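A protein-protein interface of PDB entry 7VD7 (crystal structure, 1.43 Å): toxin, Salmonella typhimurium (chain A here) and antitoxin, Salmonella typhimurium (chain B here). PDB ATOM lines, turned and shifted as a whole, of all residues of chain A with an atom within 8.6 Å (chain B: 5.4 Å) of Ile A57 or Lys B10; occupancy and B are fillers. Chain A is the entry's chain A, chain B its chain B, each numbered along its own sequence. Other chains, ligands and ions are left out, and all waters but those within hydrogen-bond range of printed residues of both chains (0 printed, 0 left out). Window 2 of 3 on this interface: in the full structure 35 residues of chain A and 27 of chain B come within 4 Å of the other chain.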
ATOM      1  N   GLY A  52      27.726  14.584 -14.709  1.00  0.00           N
ATOM      2  CA  GLY A  52      28.047  14.547 -16.152  1.00  0.00           C
ATOM      3  C   GLY A  52      26.829  14.714 -17.012  1.00  0.00           C
ATOM      4  O   GLY A  52      25.701  14.624 -16.551  1.00  0.00           O
ATOM      5  N   LEU A  53      27.090  15.000 -18.269  1.00  0.00           N
ATOM      6  CA  LEU A  53      26.046  15.244 -19.265  1.00  0.00           C
ATOM      7  C   LEU A  53      25.695  13.926 -19.943  1.00  0.00           C
ATOM      8  O   LEU A  53      26.634  13.219 -20.421  1.00  0.00           O
ATOM      9  CB  LEU A  53      26.570  16.263 -20.278  1.00  0.00           C
ATOM     10  CG  LEU A  53      25.611  16.664 -21.392  1.00  0.00           C
ATOM     11  CD1 LEU A  53      24.439  17.448 -20.827  1.00  0.00           C
ATOM     12  CD2 LEU A  53      26.355  17.494 -22.464  1.00  0.00           C
ATOM     13  N   VAL A  54      24.423  13.568 -20.022  1.00  0.00           N
ATOM     14  CA  VAL A  54      23.895  12.307 -20.599  1.00  0.00           C
ATOM     15  C   VAL A  54      23.189  12.596 -21.931  1.00  0.00           C
ATOM     16  O   VAL A  54      22.282  13.430 -21.951  1.00  0.00           O
ATOM     17  CB  VAL A  54      22.991  11.634 -19.551  1.00  0.00           C
ATOM     18  CG1 VAL A  54      22.250  10.434 -20.124  1.00  0.00           C
ATOM     19  CG2 VAL A  54      23.836  11.262 -18.325  1.00  0.00           C
ATOM     20  N   HIS A  55      23.630  11.935 -23.000  1.00  0.00           N
ATOM     21  CA  HIS A  55      23.052  12.007 -24.356  1.00  0.00           C
ATOM     22  C   HIS A  55      22.975  13.462 -24.817  1.00  0.00           C
ATOM     23  O   HIS A  55      22.075  13.796 -25.588  1.00  0.00           O
ATOM     24  CB  HIS A  55      21.707  11.263 -24.387  1.00  0.00           C
ATOM     25  CG  HIS A  55      21.792   9.778 -24.179  1.00  0.00           C
ATOM     26  ND1 HIS A  55      22.413   8.944 -25.056  1.00  0.00           N
ATOM     27  CD2 HIS A  55      21.342   9.014 -23.174  1.00  0.00           C
ATOM     28  CE1 HIS A  55      22.307   7.706 -24.604  1.00  0.00           C
ATOM     29  NE2 HIS A  55      21.658   7.719 -23.472  1.00  0.00           N
ATOM     30  N   GLY A  56      23.892  14.316 -24.404  1.00  0.00           N
ATOM     31  CA  GLY A  56      23.875  15.731 -24.766  1.00  0.00           C
ATOM     32  C   GLY A  56      22.686  16.487 -24.231  1.00  0.00           C
ATOM     33  O   GLY A  56      22.611  17.663 -24.598  1.00  0.00           O
ATOM     34  N   ILE A  57      21.822  15.899 -23.372  1.00  0.00           N
ATOM     35  CA  ILE A  57      20.464  16.448 -23.083  1.00  0.00           C
ATOM     36  C   ILE A  57      20.405  16.947 -21.636  1.00  0.00           C
ATOM     37  O   ILE A  57      19.755  17.959 -21.385  1.00  0.00           O
ATOM     38  CB  ILE A  57      19.359  15.427 -23.376  1.00  0.00           C
ATOM     39  CG1 ILE A  57      19.231  15.167 -24.873  1.00  0.00           C
ATOM     40  CG2 ILE A  57      18.046  15.874 -22.774  1.00  0.00           C
ATOM     41  CD1 ILE A  57      18.592  13.868 -25.249  1.00  0.00           C
ATOM     42  N   VAL A  58      20.986  16.238 -20.658  1.00  0.00           N
ATOM     43  CA  VAL A  58      20.746  16.614 -19.244  1.00  0.00           C
ATOM     44  C   VAL A  58      21.955  16.278 -18.376  1.00  0.00           C
ATOM     45  O   VAL A  58      22.588  15.202 -18.556  1.00  0.00           O
ATOM     46  CB  VAL A  58      19.446  15.975 -18.745  1.00  0.00           C
ATOM     47  CG1 VAL A  58      19.534  14.454 -18.813  1.00  0.00           C
ATOM     48  CG2 VAL A  58      19.051  16.494 -17.380  1.00  0.00           C
ATOM     49  N   VAL A  59      22.277  17.159 -17.471  1.00  0.00           N
ATOM     50  CA  VAL A  59      23.310  16.933 -16.439  1.00  0.00           C
ATOM     51  C   VAL A  59      22.710  16.176 -15.269  1.00  0.00           C
ATOM     52  O   VAL A  59      21.659  16.632 -14.689  1.00  0.00           O
ATOM     53  CB  VAL A  59      24.028  18.210 -16.000  1.00  0.00           C
ATOM     54  CG1 VAL A  59      25.058  17.926 -14.907  1.00  0.00           C
ATOM     55  CG2 VAL A  59      24.642  18.888 -17.234  1.00  0.00           C
ATOM     56  N   ILE A  60      23.308  15.037 -14.989  1.00  0.00           N
ATOM     57  CA  ILE A  60      22.868  14.211 -13.853  1.00  0.00           C
ATOM     58  C   ILE A  60      23.968  14.094 -12.822  1.00  0.00           C
ATOM     59  O   ILE A  60      25.143  14.173 -13.127  1.00  0.00           O
ATOM     60  CB  ILE A  60      22.314  12.874 -14.363  1.00  0.00           C
ATOM     61  CG1 ILE A  60      23.385  12.046 -15.008  1.00  0.00           C
ATOM     62  CG2 ILE A  60      21.073  13.037 -15.232  1.00  0.00           C
ATOM     63  CD1 ILE A  60      22.969  10.592 -15.103  1.00  0.00           C
ATOM     64  N   LYS A  82      18.574  14.308 -11.360  1.00  0.00           N
ATOM     65  CA  LYS A  82      18.962  15.527 -12.091  1.00  0.00           C
ATOM     66  C   LYS A  82      19.820  16.427 -11.203  1.00  0.00           C
ATOM     67  O   LYS A  82      19.568  16.570  -9.979  1.00  0.00           O
ATOM     68  CB  LYS A  82      17.719  16.299 -12.529  1.00  0.00           C
ATOM     69  CG  LYS A  82      17.996  17.460 -13.455  1.00  0.00           C
ATOM     70  CD  LYS A  82      16.772  18.195 -13.936  1.00  0.00           C
ATOM     71  CE  LYS A  82      17.083  19.184 -15.055  1.00  0.00           C
ATOM     72  NZ  LYS A  82      18.013  20.239 -14.604  1.00  0.00           N
ATOM     73  N   ARG A  88      24.964  22.114 -11.540  1.00  0.00           N
ATOM     74  CA  ARG A  88      25.195  22.494 -12.955  1.00  0.00           C
ATOM     75  C   ARG A  88      26.302  23.559 -13.031  1.00  0.00           C
ATOM     76  O   ARG A  88      27.151  23.476 -13.916  1.00  0.00           O
ATOM     77  CB  ARG A  88      23.907  22.968 -13.600  1.00  0.00           C
ATOM     78  CG  ARG A  88      22.860  21.876 -13.770  1.00  0.00           C
ATOM     79  CD  ARG A  88      21.696  22.346 -14.617  1.00  0.00           C
ATOM     80  NE  ARG A  88      20.995  23.501 -14.039  1.00  0.00           N
ATOM     81  CZ  ARG A  88      19.987  23.453 -13.173  1.00  0.00           C
ATOM     82  NH1 ARG A  88      19.456  22.301 -12.774  1.00  0.00           N
ATOM     83  NH2 ARG A  88      19.437  24.592 -12.787  1.00  0.00           N
ATOM     84  N   HIS B   5      12.685   6.935 -25.322  1.00  0.00           N
ATOM     85  CA  HIS B   5      13.835   7.198 -24.416  1.00  0.00           C
ATOM     86  C   HIS B   5      14.272   8.646 -24.546  1.00  0.00           C
ATOM     87  O   HIS B   5      14.538   9.329 -23.558  1.00  0.00           O
ATOM     88  CB  HIS B   5      14.956   6.204 -24.683  1.00  0.00           C
ATOM     89  CG  HIS B   5      15.993   6.166 -23.622  1.00  0.00           C
ATOM     90  ND1 HIS B   5      17.035   5.268 -23.717  1.00  0.00           N
ATOM     91  CD2 HIS B   5      16.217   6.929 -22.530  1.00  0.00           C
ATOM     92  CE1 HIS B   5      17.836   5.475 -22.691  1.00  0.00           C
ATOM     93  NE2 HIS B   5      17.337   6.452 -21.957  1.00  0.00           N
ATOM     94  N   GLU B   6      14.416   9.123 -25.781  1.00  0.00           N
ATOM     95  CA  GLU B   6      14.766  10.544 -25.986  1.00  0.00           C
ATOM     96  C   GLU B   6      13.767  11.476 -25.298  1.00  0.00           C
ATOM     97  O   GLU B   6      14.203  12.455 -24.616  1.00  0.00           O
ATOM     98  CB  GLU B   6      14.940  10.839 -27.481  1.00  0.00           C
ATOM     99  CG  GLU B   6      15.385  12.271 -27.753  1.00  0.00           C
ATOM    100  CD  GLU B   6      15.866  12.545 -29.176  1.00  0.00           C
ATOM    101  OE1 GLU B   6      15.320  11.928 -30.125  1.00  0.00           O
ATOM    102  OE2 GLU B   6      16.789  13.378 -29.338  1.00  0.00           O
ATOM    103  N   ALA B   7      12.487  11.179 -25.457  1.00  0.00           N
ATOM    104  CA  ALA B   7      11.424  11.976 -24.805  1.00  0.00           C
ATOM    105  C   ALA B   7      11.608  11.974 -23.270  1.00  0.00           C
ATOM    106  O   ALA B   7      11.405  13.033 -22.651  1.00  0.00           O
ATOM    107  CB  ALA B   7      10.075  11.431 -25.210  1.00  0.00           C
ATOM    108  N   GLU B   8      11.976  10.847 -22.666  1.00  0.00           N
ATOM    109  CA  GLU B   8      12.136  10.815 -21.190  1.00  0.00           C
ATOM    110  C   GLU B   8      13.240  11.817 -20.809  1.00  0.00           C
ATOM    111  O   GLU B   8      13.123  12.526 -19.820  1.00  0.00           O
ATOM    112  CB  GLU B   8      12.634   9.474 -20.674  1.00  0.00           C
ATOM    113  CG  GLU B   8      11.605   8.364 -20.705  1.00  0.00           C
ATOM    114  CD  GLU B   8      12.144   7.028 -20.219  1.00  0.00           C
ATOM    115  OE1 GLU B   8      13.381   6.901 -19.956  1.00  0.00           O
ATOM    116  OE2 GLU B   8      11.369   6.074 -20.149  1.00  0.00           O
ATOM    117  N   LEU B   9      14.309  11.893 -21.610  1.00  0.00           N
ATOM    118  CA  LEU B   9      15.489  12.705 -21.245  1.00  0.00           C
ATOM    119  C   LEU B   9      15.152  14.172 -21.472  1.00  0.00           C
ATOM    120  O   LEU B   9      15.565  15.026 -20.654  1.00  0.00           O
ATOM    121  CB  LEU B   9      16.695  12.274 -22.065  1.00  0.00           C
ATOM    122  CG  LEU B   9      17.211  10.896 -21.684  1.00  0.00           C
ATOM    123  CD1 LEU B   9      18.222  10.454 -22.729  1.00  0.00           C
ATOM    124  CD2 LEU B   9      17.819  10.870 -20.286  1.00  0.00           C
ATOM    125  N   LYS B  10      14.384  14.449 -22.498  1.00  0.00           N
ATOM    126  CA  LYS B  10      13.968  15.846 -22.738  1.00  0.00           C
ATOM    127  C   LYS B  10      13.000  16.331 -21.652  1.00  0.00           C
ATOM    128  O   LYS B  10      13.139  17.456 -21.253  1.00  0.00           O
ATOM    129  CB  LYS B  10      13.371  15.977 -24.137  1.00  0.00           C
ATOM    130  CG  LYS B  10      14.408  16.275 -25.208  1.00  0.00           C
ATOM    131  CD  LYS B  10      14.102  15.611 -26.514  1.00  0.00           C
ATOM    132  CE  LYS B  10      15.056  16.025 -27.613  1.00  0.00           C
ATOM    133  NZ  LYS B  10      14.377  16.918 -28.575  1.00  0.00           N
ATOM    134  N   ALA B  11      12.109  15.480 -21.164  1.00  0.00           N
ATOM    135  CA  ALA B  11      11.215  15.808 -20.020  1.00  0.00           C
ATOM    136  C   ALA B  11      12.084  16.087 -18.793  1.00  0.00           C
ATOM    137  O   ALA B  11      11.861  17.107 -18.089  1.00  0.00           O
ATOM    138  CB  ALA B  11      10.254  14.690 -19.767  1.00  0.00           C
ATOM    139  N   LEU B  12      13.080  15.242 -18.539  1.00  0.00           N
ATOM    140  CA  LEU B  12      13.949  15.447 -17.362  1.00  0.00           C
ATOM    141  C   LEU B  12      14.676  16.792 -17.500  1.00  0.00           C
ATOM    142  O   LEU B  12      14.782  17.501 -16.464  1.00  0.00           O
ATOM    143  CB  LEU B  12      14.875  14.236 -17.228  1.00  0.00           C
ATOM    144  CG  LEU B  12      15.729  14.226 -15.965  1.00  0.00           C
ATOM    145  CD1 LEU B  12      14.860  14.003 -14.754  1.00  0.00           C
ATOM    146  CD2 LEU B  12      16.831  13.175 -16.022  1.00  0.00           C
ATOM    147  N   ALA B  13      15.119  17.145 -18.709  1.00  0.00           N
ATOM    148  CA  ALA B  13      15.865  18.395 -19.001  1.00  0.00           C
ATOM    149  C   ALA B  13      14.994  19.625 -18.678  1.00  0.00           C
ATOM    150  O   ALA B  13      15.571  20.666 -18.295  1.00  0.00           O
ATOM    151  CB  ALA B  13      16.320  18.425 -20.430  1.00  0.00           C
ATOM    152  N   LYS B  14      13.679  19.489 -18.809  1.00  0.00           N
ATOM    153  CA  LYS B  14      12.694  20.591 -18.550  1.00  0.00           C
ATOM    154  C   LYS B  14      12.215  20.609 -17.087  1.00  0.00           C
ATOM    155  O   LYS B  14      11.401  21.489 -16.743  1.00  0.00           O
ATOM    156  CB  LYS B  14      11.465  20.425 -19.447  1.00  0.00           C
ATOM    157  CG  LYS B  14      11.700  20.680 -20.921  1.00  0.00           C
ATOM    158  CD  LYS B  14      10.434  20.567 -21.734  1.00  0.00           C
ATOM    159  CE  LYS B  14      10.429  19.372 -22.656  1.00  0.00           C
ATOM    160  NZ  LYS B  14      11.311  19.595 -23.821  1.00  0.00           N
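His A55 touches Leu B9 (CD2 to CD1, 3.5 Å).
O of Leu B9 touches CG2 of Ile A57, 3.4 Å away.
Ile A57 touches Lys B10.
Ile A57 touches Ala B13 (O to CB, 3.6 Å).
Leu B12 touches Lys A82.
Ala B13 touches Lys A82.
Printed residues of chain B within 4 Å of Ile A57: Leu B9 (3.4 Å), Lys B10 (3.9 Å) and Ala B13 (3.6 Å).
Val A59 touches none of the printed residues of chain B.
Printed residues of chain B within 4 Å of Lys A82: Leu B12 (3.2 Å) and Ala B13 (3.9 Å).
Ala B7 touches none of the printed residues of chain A.
Printed residues of chain A within 4 Å of Leu B9: His A55 and Ile A57.
Lys B10 touches just one residue of chain A: Ile A57.
No residue of chain A comes within 4 Å of Ala B11.
Of the 11 printed residues of chain A, 3 touch a printed residue of chain B.
Hydrophobic or aromatic side chains of chain A within 4 Å of the printed part of chain B: His A55 and Ile A57.
Among the printed residues, no Asp or Glu carboxylate lies within 4 Å of a Lys or Arg side-chain nitrogen of the other chain.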
